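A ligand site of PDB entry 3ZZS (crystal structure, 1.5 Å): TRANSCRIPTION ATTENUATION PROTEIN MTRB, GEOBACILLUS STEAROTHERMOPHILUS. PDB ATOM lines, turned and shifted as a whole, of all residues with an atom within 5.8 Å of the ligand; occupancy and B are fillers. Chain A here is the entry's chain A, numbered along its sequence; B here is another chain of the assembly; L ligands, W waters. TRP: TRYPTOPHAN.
Merely in contact with the ligand: Arg 20 (3.5 Å), Gly 17 of chain B (3.5 Å), His 45 of chain B (3.8 Å), Ala 40 of chain B (3.8 Å), Ile 49 of chain B (3.9 Å), His 27 of chain B (3.9 Å) and His 28 of chain B (3.96 Å). Within 4 Å of the ligand: Thr 19, Arg 20, Gly 21, Asp 23, Thr 24, Ser 47, Gly 17 of chain B, His 27 of chain B, His 28 of chain B, Ala 40 of chain B, Gln 41 of chain B, Thr 43 of chain B, His 45 of chain B, Thr 46 of chain B and Ile 49 of chain B.
Water W1 lies within hydrogen-bond range of ND1 of His 45 of chain B, O of the ligand, OG1 of Thr 43 of chain B and N of Gly 21.
OG1 of Thr 43 of chain B is in hydrogen-bond range of OXT of the ligand (2.6 Å). The backbone carbonyl oxygen (O) of Thr 19 is in hydrogen-bond range of a nitrogen (N) of the ligand, at 2.8 Å. N of Gly 21 is in hydrogen-bond range of O of the ligand (3.1 Å). O of Gly 21 is in hydrogen-bond range of N of the ligand (2.8 Å). OG1 of Thr 46 of chain B lies within hydrogen-bond range of OXT of the ligand. OG1 of Thr 24 is in hydrogen-bond range of N of the ligand (2.8 Å). O of Gln 41 of chain B is in hydrogen-bond range of NE1 of the ligand. OG of Ser 47 is in hydrogen-bond range of O of the ligand, 2.9 Å away. O of Asp 23 lies within hydrogen-bond range of N of the ligand, 3.1 Å away.
The backbone NH (N) of His 45 of chain B sits at hydrogen-bond distance from the side-chain hydroxyl (OG1) of Thr 43 of chain B, at 3.1 Å. The side-chain hydroxyl of Thr 19 sits at hydrogen-bond distance from the backbone carbonyl oxygen of Asp 23, 3.0 Å away. OG1 of Thr 46 of chain B is in hydrogen-bond range of NE2 of His 27 of chain B (2.7 Å). The backbone NH (N) of Gln 41 of chain B is in hydrogen-bond range of the backbone carbonyl oxygen (O) of Ser 47, at 3.0 Å. The side-chain amide oxygen of Gln 41 of chain B is in hydrogen-bond range of the guanidinium group of Arg 20 (2.7 Å). The backbone NH (N) of Ser 47 lies within hydrogen-bond range of the backbone carbonyl oxygen (O) of Leu 18 of chain A, 3.2 Å away. The backbone carbonyl oxygen of His 28 of chain B sits at hydrogen-bond distance from the backbone NH of Gly 17 of chain B, 2.9 Å away. A ring nitrogen (NE2) of His 28 of chain B sits at hydrogen-bond distance from the side-chain carboxylate (OE1) of Glu 30 of chain B, at 2.8 Å.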
ATOM      1  N   LEU A  18      -1.444  22.172  -3.583  1.00  0.00           N
ATOM      2  CA  LEU A  18      -0.537  22.622  -4.733  1.00  0.00           C
ATOM      3  C   LEU A  18       0.581  21.589  -4.862  1.00  0.00           C
ATOM      4  O   LEU A  18       1.066  21.028  -3.878  1.00  0.00           O
ATOM      5  CB  LEU A  18       0.115  23.982  -4.466  1.00  0.00           C
ATOM      6  CG  LEU A  18      -0.744  25.232  -4.644  1.00  0.00           C
ATOM      7  CD1 LEU A  18      -1.781  25.327  -3.548  1.00  0.00           C
ATOM      8  CD2 LEU A  18       0.122  26.486  -4.646  1.00  0.00           C
ATOM      9  N   THR A  19       0.901  21.257  -6.112  1.00  0.00           N
ATOM     10  CA  THR A  19       1.849  20.203  -6.412  1.00  0.00           C
ATOM     11  C   THR A  19       3.264  20.475  -5.907  1.00  0.00           C
ATOM     12  O   THR A  19       3.821  21.552  -6.119  1.00  0.00           O
ATOM     13  CB  THR A  19       1.963  19.955  -7.923  1.00  0.00           C
ATOM     14  OG1 THR A  19       2.311  21.191  -8.589  1.00  0.00           O
ATOM     15  CG2 THR A  19       0.654  19.403  -8.489  1.00  0.00           C
ATOM     16  N   ARG A  20       3.855  19.467  -5.263  1.00  0.00           N
ATOM     17  CA  ARG A  20       5.263  19.475  -4.962  1.00  0.00           C
ATOM     18  C   ARG A  20       6.058  19.273  -6.249  1.00  0.00           C
ATOM     19  O   ARG A  20       5.690  18.447  -7.079  1.00  0.00           O
ATOM     20  CB  ARG A  20       5.606  18.368  -3.965  1.00  0.00           C
ATOM     21  CG  ARG A  20       7.104  18.312  -3.581  1.00  0.00           C
ATOM     22  CD  ARG A  20       7.422  17.220  -2.552  1.00  0.00           C
ATOM     23  NE  ARG A  20       6.625  17.358  -1.341  1.00  0.00           N
ATOM     24  CZ  ARG A  20       6.908  18.175  -0.328  1.00  0.00           C
ATOM     25  NH1 ARG A  20       7.987  18.949  -0.348  1.00  0.00           N
ATOM     26  NH2 ARG A  20       6.078  18.221   0.711  1.00  0.00           N
ATOM     27  N   GLY A  21       7.131  20.040  -6.416  1.00  0.00           N
ATOM     28  CA  GLY A  21       8.060  19.862  -7.527  1.00  0.00           C
ATOM     29  C   GLY A  21       8.410  21.166  -8.211  1.00  0.00           C
ATOM     30  O   GLY A  21       8.090  22.254  -7.722  1.00  0.00           O
ATOM     31  N   ALA A  22       9.079  21.059  -9.348  1.00  0.00           N
ATOM     32  CA  ALA A  22       9.501  22.237 -10.094  1.00  0.00           C
ATOM     33  C   ALA A  22       8.302  23.056 -10.561  1.00  0.00           C
ATOM     34  O   ALA A  22       8.369  24.280 -10.602  1.00  0.00           O
ATOM     35  CB  ALA A  22      10.361  21.828 -11.297  1.00  0.00           C
ATOM     36  N   ASP A  23       7.226  22.354 -10.921  1.00  0.00           N
ATOM     37  CA  ASP A  23       5.995  23.013 -11.374  1.00  0.00           C
ATOM     38  C   ASP A  23       5.007  23.156 -10.235  1.00  0.00           C
ATOM     39  O   ASP A  23       4.974  22.348  -9.309  1.00  0.00           O
ATOM     40  CB  ASP A  23       5.353  22.222 -12.519  1.00  0.00           C
ATOM     41  CG  ASP A  23       6.167  22.267 -13.804  1.00  0.00           C
ATOM     42  OD1 ASP A  23       7.008  23.162 -13.974  1.00  0.00           O
ATOM     43  OD2 ASP A  23       5.945  21.380 -14.654  1.00  0.00           O
ATOM     44  N   THR A  24       4.193  24.208 -10.304  1.00  0.00           N
ATOM     45  CA  THR A  24       3.176  24.487  -9.296  1.00  0.00           C
ATOM     46  C   THR A  24       1.820  24.674  -9.960  1.00  0.00           C
ATOM     47  O   THR A  24       1.605  25.608 -10.733  1.00  0.00           O
ATOM     48  CB  THR A  24       3.527  25.742  -8.493  1.00  0.00           C
ATOM     49  OG1 THR A  24       4.856  25.601  -7.964  1.00  0.00           O
ATOM     50  CG2 THR A  24       2.551  25.971  -7.355  1.00  0.00           C
ATOM     51  N   SER A  47       2.941  20.305  -1.335  1.00  0.00           N
ATOM     52  CA  SER A  47       3.917  21.112  -0.592  1.00  0.00           C
ATOM     53  C   SER A  47       3.419  22.530  -0.266  1.00  0.00           C
ATOM     54  O   SER A  47       4.163  23.310   0.349  1.00  0.00           O
ATOM     55  CB  SER A  47       5.225  21.199  -1.371  1.00  0.00           C
ATOM     56  OG  SER A  47       5.010  21.871  -2.600  1.00  0.00           O
ATOM     57  N   ALA A  48       2.198  22.856  -0.668  1.00  0.00           N
ATOM     58  CA  ALA A  48       1.548  24.101  -0.269  1.00  0.00           C
ATOM     59  C   ALA A  48       0.052  23.883  -0.302  1.00  0.00           C
ATOM     60  O   ALA A  48      -0.448  23.116  -1.130  1.00  0.00           O
ATOM     61  CB  ALA A  48       1.955  25.253  -1.179  1.00  0.00           C
ATOM     62  N   VAL B  15       2.632  35.786  -3.339  1.00  0.00           N
ATOM     63  CA  VAL B  15       3.583  34.923  -2.648  1.00  0.00           C
ATOM     64  C   VAL B  15       4.420  34.255  -3.724  1.00  0.00           C
ATOM     65  O   VAL B  15       3.897  33.517  -4.548  1.00  0.00           O
ATOM     66  CB  VAL B  15       2.901  33.876  -1.744  1.00  0.00           C
ATOM     67  CG1 VAL B  15       3.949  33.003  -1.032  1.00  0.00           C
ATOM     68  CG2 VAL B  15       1.987  34.553  -0.722  1.00  0.00           C
ATOM     69  N   ILE B  16       5.719  34.552  -3.717  1.00  0.00           N
ATOM     70  CA  ILE B  16       6.601  34.230  -4.823  1.00  0.00           C
ATOM     71  C   ILE B  16       7.650  33.222  -4.357  1.00  0.00           C
ATOM     72  O   ILE B  16       8.344  33.463  -3.366  1.00  0.00           O
ATOM     73  CB  ILE B  16       7.311  35.494  -5.361  1.00  0.00           C
ATOM     74  CG1 ILE B  16       6.309  36.589  -5.747  1.00  0.00           C
ATOM     75  CG2 ILE B  16       8.204  35.142  -6.554  1.00  0.00           C
ATOM     76  CD1 ILE B  16       6.913  37.959  -5.789  1.00  0.00           C
ATOM     77  N   GLY B  17       7.762  32.097  -5.055  1.00  0.00           N
ATOM     78  CA  GLY B  17       8.787  31.106  -4.738  1.00  0.00           C
ATOM     79  C   GLY B  17      10.054  31.350  -5.540  1.00  0.00           C
ATOM     80  O   GLY B  17       9.991  31.514  -6.767  1.00  0.00           O
ATOM     81  N   LEU B  18      11.185  31.377  -4.852  1.00  0.00           N
ATOM     82  CA  LEU B  18      12.503  31.534  -5.465  1.00  0.00           C
ATOM     83  C   LEU B  18      13.184  30.174  -5.557  1.00  0.00           C
ATOM     84  O   LEU B  18      13.148  29.365  -4.617  1.00  0.00           O
ATOM     85  CB  LEU B  18      13.399  32.508  -4.689  1.00  0.00           C
ATOM     86  CG  LEU B  18      13.109  34.008  -4.797  1.00  0.00           C
ATOM     87  CD1 LEU B  18      11.755  34.357  -4.204  1.00  0.00           C
ATOM     88  CD2 LEU B  18      14.219  34.816  -4.112  1.00  0.00           C
ATOM     89  N   HIS B  27      10.051  31.140  -9.691  1.00  0.00           N
ATOM     90  CA  HIS B  27       9.460  30.035 -10.447  1.00  0.00           C
ATOM     91  C   HIS B  27       7.932  29.997 -10.355  1.00  0.00           C
ATOM     92  O   HIS B  27       7.292  29.345 -11.180  1.00  0.00           O
ATOM     93  CB  HIS B  27      10.041  28.670 -10.039  1.00  0.00           C
ATOM     94  CG  HIS B  27       9.749  28.274  -8.623  1.00  0.00           C
ATOM     95  ND1 HIS B  27       8.514  27.818  -8.216  1.00  0.00           N
ATOM     96  CD2 HIS B  27      10.538  28.275  -7.527  1.00  0.00           C
ATOM     97  CE1 HIS B  27       8.554  27.551  -6.920  1.00  0.00           C
ATOM     98  NE2 HIS B  27       9.769  27.817  -6.483  1.00  0.00           N
ATOM     99  N   HIS B  28       7.361  30.689  -9.370  1.00  0.00           N
ATOM    100  CA  HIS B  28       5.920  30.700  -9.212  1.00  0.00           C
ATOM    101  C   HIS B  28       5.490  31.909  -8.409  1.00  0.00           C
ATOM    102  O   HIS B  28       6.120  32.240  -7.421  1.00  0.00           O
ATOM    103  CB  HIS B  28       5.429  29.437  -8.501  1.00  0.00           C
ATOM    104  CG  HIS B  28       3.947  29.387  -8.356  1.00  0.00           C
ATOM    105  ND1 HIS B  28       3.112  29.131  -9.417  1.00  0.00           N
ATOM    106  CD2 HIS B  28       3.136  29.599  -7.282  1.00  0.00           C
ATOM    107  CE1 HIS B  28       1.847  29.175  -9.007  1.00  0.00           C
ATOM    108  NE2 HIS B  28       1.841  29.462  -7.723  1.00  0.00           N
ATOM    109  N   SER B  29       4.400  32.528  -8.846  1.00  0.00           N
ATOM    110  CA  SER B  29       3.751  33.591  -8.092  1.00  0.00           C
ATOM    111  C   SER B  29       2.325  33.175  -7.807  1.00  0.00           C
ATOM    112  O   SER B  29       1.532  32.983  -8.739  1.00  0.00           O
ATOM    113  CB  SER B  29       3.769  34.877  -8.911  1.00  0.00           C
ATOM    114  OG  SER B  29       3.031  35.890  -8.253  1.00  0.00           O
ATOM    115  N   GLU B  30       1.988  33.022  -6.527  1.00  0.00           N
ATOM    116  CA  GLU B  30       0.634  32.688  -6.127  1.00  0.00           C
ATOM    117  C   GLU B  30      -0.060  33.957  -5.671  1.00  0.00           C
ATOM    118  O   GLU B  30       0.369  34.591  -4.714  1.00  0.00           O
ATOM    119  CB  GLU B  30       0.628  31.648  -5.010  1.00  0.00           C
ATOM    120  CG  GLU B  30      -0.758  31.106  -4.657  1.00  0.00           C
ATOM    121  CD  GLU B  30      -1.406  30.328  -5.802  1.00  0.00           C
ATOM    122  OE1 GLU B  30      -0.673  29.699  -6.602  1.00  0.00           O
ATOM    123  OE2 GLU B  30      -2.643  30.350  -5.910  1.00  0.00           O
ATOM    124  N   LEU B  38      -2.341  31.012   2.427  1.00  0.00           N
ATOM    125  CA  LEU B  38      -1.439  30.044   1.838  1.00  0.00           C
ATOM    126  C   LEU B  38      -0.522  29.520   2.923  1.00  0.00           C
ATOM    127  O   LEU B  38       0.099  30.313   3.663  1.00  0.00           O
ATOM    128  CB  LEU B  38      -0.614  30.670   0.714  1.00  0.00           C
ATOM    129  CG  LEU B  38       0.248  29.689  -0.095  1.00  0.00           C
ATOM    130  CD1 LEU B  38      -0.610  28.696  -0.907  1.00  0.00           C
ATOM    131  CD2 LEU B  38       1.222  30.456  -1.011  1.00  0.00           C
ATOM    132  N   ALA B  40       2.707  27.302   3.066  1.00  0.00           N
ATOM    133  CA  ALA B  40       3.686  26.905   2.072  1.00  0.00           C
ATOM    134  C   ALA B  40       4.982  26.425   2.709  1.00  0.00           C
ATOM    135  O   ALA B  40       5.552  27.113   3.548  1.00  0.00           O
ATOM    136  CB  ALA B  40       3.977  28.067   1.129  1.00  0.00           C
ATOM    137  N   GLN B  41       5.428  25.235   2.302  1.00  0.00           N
ATOM    138  CA  GLN B  41       6.712  24.700   2.758  1.00  0.00           C
ATOM    139  C   GLN B  41       7.901  25.249   1.997  1.00  0.00           C
ATOM    140  O   GLN B  41       7.798  25.678   0.854  1.00  0.00           O
ATOM    141  CB  GLN B  41       6.720  23.189   2.606  1.00  0.00           C
ATOM    142  CG  GLN B  41       5.830  22.467   3.558  1.00  0.00           C
ATOM    143  CD  GLN B  41       5.931  20.981   3.392  1.00  0.00           C
ATOM    144  OE1 GLN B  41       5.774  20.454   2.284  1.00  0.00           O
ATOM    145  NE2 GLN B  41       6.214  20.276   4.482  1.00  0.00           N
ATOM    146  N   PHE B  42       9.062  25.217   2.653  1.00  0.00           N
ATOM    147  CA  PHE B  42      10.326  25.178   1.924  1.00  0.00           C
ATOM    148  C   PHE B  42      10.507  23.754   1.387  1.00  0.00           C
ATOM    149  O   PHE B  42      10.108  22.791   2.033  1.00  0.00           O
ATOM    150  CB  PHE B  42      11.494  25.593   2.822  1.00  0.00           C
ATOM    151  CG  PHE B  42      11.483  27.041   3.166  1.00  0.00           C
ATOM    152  CD1 PHE B  42      11.752  27.984   2.192  1.00  0.00           C
ATOM    153  CD2 PHE B  42      11.163  27.479   4.436  1.00  0.00           C
ATOM    154  CE1 PHE B  42      11.731  29.323   2.471  1.00  0.00           C
ATOM    155  CE2 PHE B  42      11.152  28.821   4.718  1.00  0.00           C
ATOM    156  CZ  PHE B  42      11.443  29.741   3.733  1.00  0.00           C
ATOM    157  N   THR B  43      11.073  23.638   0.196  1.00  0.00           N
ATOM    158  CA  THR B  43      11.057  22.378  -0.538  1.00  0.00           C
ATOM    159  C   THR B  43      12.324  22.209  -1.352  1.00  0.00           C
ATOM    160  O   THR B  43      13.193  23.088  -1.386  1.00  0.00           O
ATOM    161  CB  THR B  43       9.883  22.371  -1.525  1.00  0.00           C
ATOM    162  OG1 THR B  43      10.200  23.314  -2.561  1.00  0.00           O
ATOM    163  CG2 THR B  43       8.531  22.752  -0.858  1.00  0.00           C
ATOM    164  N   GLU B  44      12.417  21.085  -2.062  1.00  0.00           N
ATOM    165  CA  GLU B  44      13.513  20.853  -2.977  1.00  0.00           C
ATOM    166  C   GLU B  44      13.662  21.984  -4.006  1.00  0.00           C
ATOM    167  O   GLU B  44      14.767  22.289  -4.421  1.00  0.00           O
ATOM    168  CB  GLU B  44      13.315  19.520  -3.705  1.00  0.00           C
ATOM    169  CG  GLU B  44      14.358  19.205  -4.724  1.00  0.00           C
ATOM    170  CD  GLU B  44      14.161  17.859  -5.394  1.00  0.00           C
ATOM    171  OE1 GLU B  44      13.242  17.101  -5.025  1.00  0.00           O
ATOM    172  OE2 GLU B  44      14.953  17.563  -6.310  1.00  0.00           O
ATOM    173  N   HIS B  45      12.541  22.594  -4.392  1.00  0.00           N
ATOM    174  CA  HIS B  45      12.553  23.608  -5.451  1.00  0.00           C
ATOM    175  C   HIS B  45      12.444  25.049  -4.962  1.00  0.00           C
ATOM    176  O   HIS B  45      12.706  25.958  -5.728  1.00  0.00           O
ATOM    177  CB  HIS B  45      11.460  23.269  -6.451  1.00  0.00           C
ATOM    178  CG  HIS B  45      11.739  21.987  -7.154  1.00  0.00           C
ATOM    179  ND1 HIS B  45      11.261  20.779  -6.713  1.00  0.00           N
ATOM    180  CD2 HIS B  45      12.559  21.704  -8.201  1.00  0.00           C
ATOM    181  CE1 HIS B  45      11.714  19.812  -7.478  1.00  0.00           C
ATOM    182  NE2 HIS B  45      12.512  20.344  -8.395  1.00  0.00           N
ATOM    183  N   THR B  46      12.078  25.252  -3.692  1.00  0.00           N
ATOM    184  CA  THR B  46      11.839  26.575  -3.122  1.00  0.00           C
ATOM    185  C   THR B  46      12.652  26.748  -1.846  1.00  0.00           C
ATOM    186  O   THR B  46      12.364  26.107  -0.840  1.00  0.00           O
ATOM    187  CB  THR B  46      10.351  26.791  -2.813  1.00  0.00           C
ATOM    188  OG1 THR B  46       9.589  26.646  -4.026  1.00  0.00           O
ATOM    189  CG2 THR B  46      10.117  28.176  -2.225  1.00  0.00           C
ATOM    190  N   ALA B  48      13.546  30.154  -0.842  1.00  0.00           N
ATOM    191  CA  ALA B  48      13.223  31.489  -0.349  1.00  0.00           C
ATOM    192  C   ALA B  48      11.838  31.859  -0.859  1.00  0.00           C
ATOM    193  O   ALA B  48      11.435  31.417  -1.938  1.00  0.00           O
ATOM    194  CB  ALA B  48      14.271  32.502  -0.778  1.00  0.00           C
ATOM    195  N   ILE B  49      11.121  32.628  -0.062  1.00  0.00           N
ATOM    196  CA  ILE B  49       9.740  33.013  -0.345  1.00  0.00           C
ATOM    197  C   ILE B  49       9.627  34.519  -0.159  1.00  0.00           C
ATOM    198  O   ILE B  49       9.995  35.044   0.895  1.00  0.00           O
ATOM    199  CB  ILE B  49       8.740  32.282   0.581  1.00  0.00           C
ATOM    200  CG1 ILE B  49       8.812  30.768   0.349  1.00  0.00           C
ATOM    201  CG2 ILE B  49       7.318  32.797   0.361  1.00  0.00           C
ATOM    202  CD1 ILE B  49       8.022  29.926   1.340  1.00  0.00           C
HETATM  203  N   TRP L   1       5.846  23.363  -6.547  1.00  0.00           N
HETATM  204  CA  TRP L   1       6.326  24.231  -5.436  1.00  0.00           C
HETATM  205  C   TRP L   1       7.393  23.495  -4.647  1.00  0.00           C
HETATM  206  O   TRP L   1       7.246  22.295  -4.362  1.00  0.00           O
HETATM  207  CB  TRP L   1       5.172  24.630  -4.533  1.00  0.00           C
HETATM  208  CG  TRP L   1       5.555  25.545  -3.449  1.00  0.00           C
HETATM  209  CD1 TRP L   1       5.904  25.215  -2.165  1.00  0.00           C
HETATM  210  CD2 TRP L   1       5.674  26.981  -3.526  1.00  0.00           C
HETATM  211  NE1 TRP L   1       6.226  26.336  -1.448  1.00  0.00           N
HETATM  212  CE2 TRP L   1       6.091  27.433  -2.253  1.00  0.00           C
HETATM  213  CE3 TRP L   1       5.449  27.920  -4.533  1.00  0.00           C
HETATM  214  CZ2 TRP L   1       6.287  28.774  -1.968  1.00  0.00           C
HETATM  215  CZ3 TRP L   1       5.654  29.264  -4.246  1.00  0.00           C
HETATM  216  CH2 TRP L   1       6.076  29.680  -2.981  1.00  0.00           C
HETATM  217  OXT TRP L   1       8.408  24.093  -4.284  1.00  0.00           O
HETATM  218  O   HOH W   1       9.684  20.750  -4.439  1.00  0.00           O
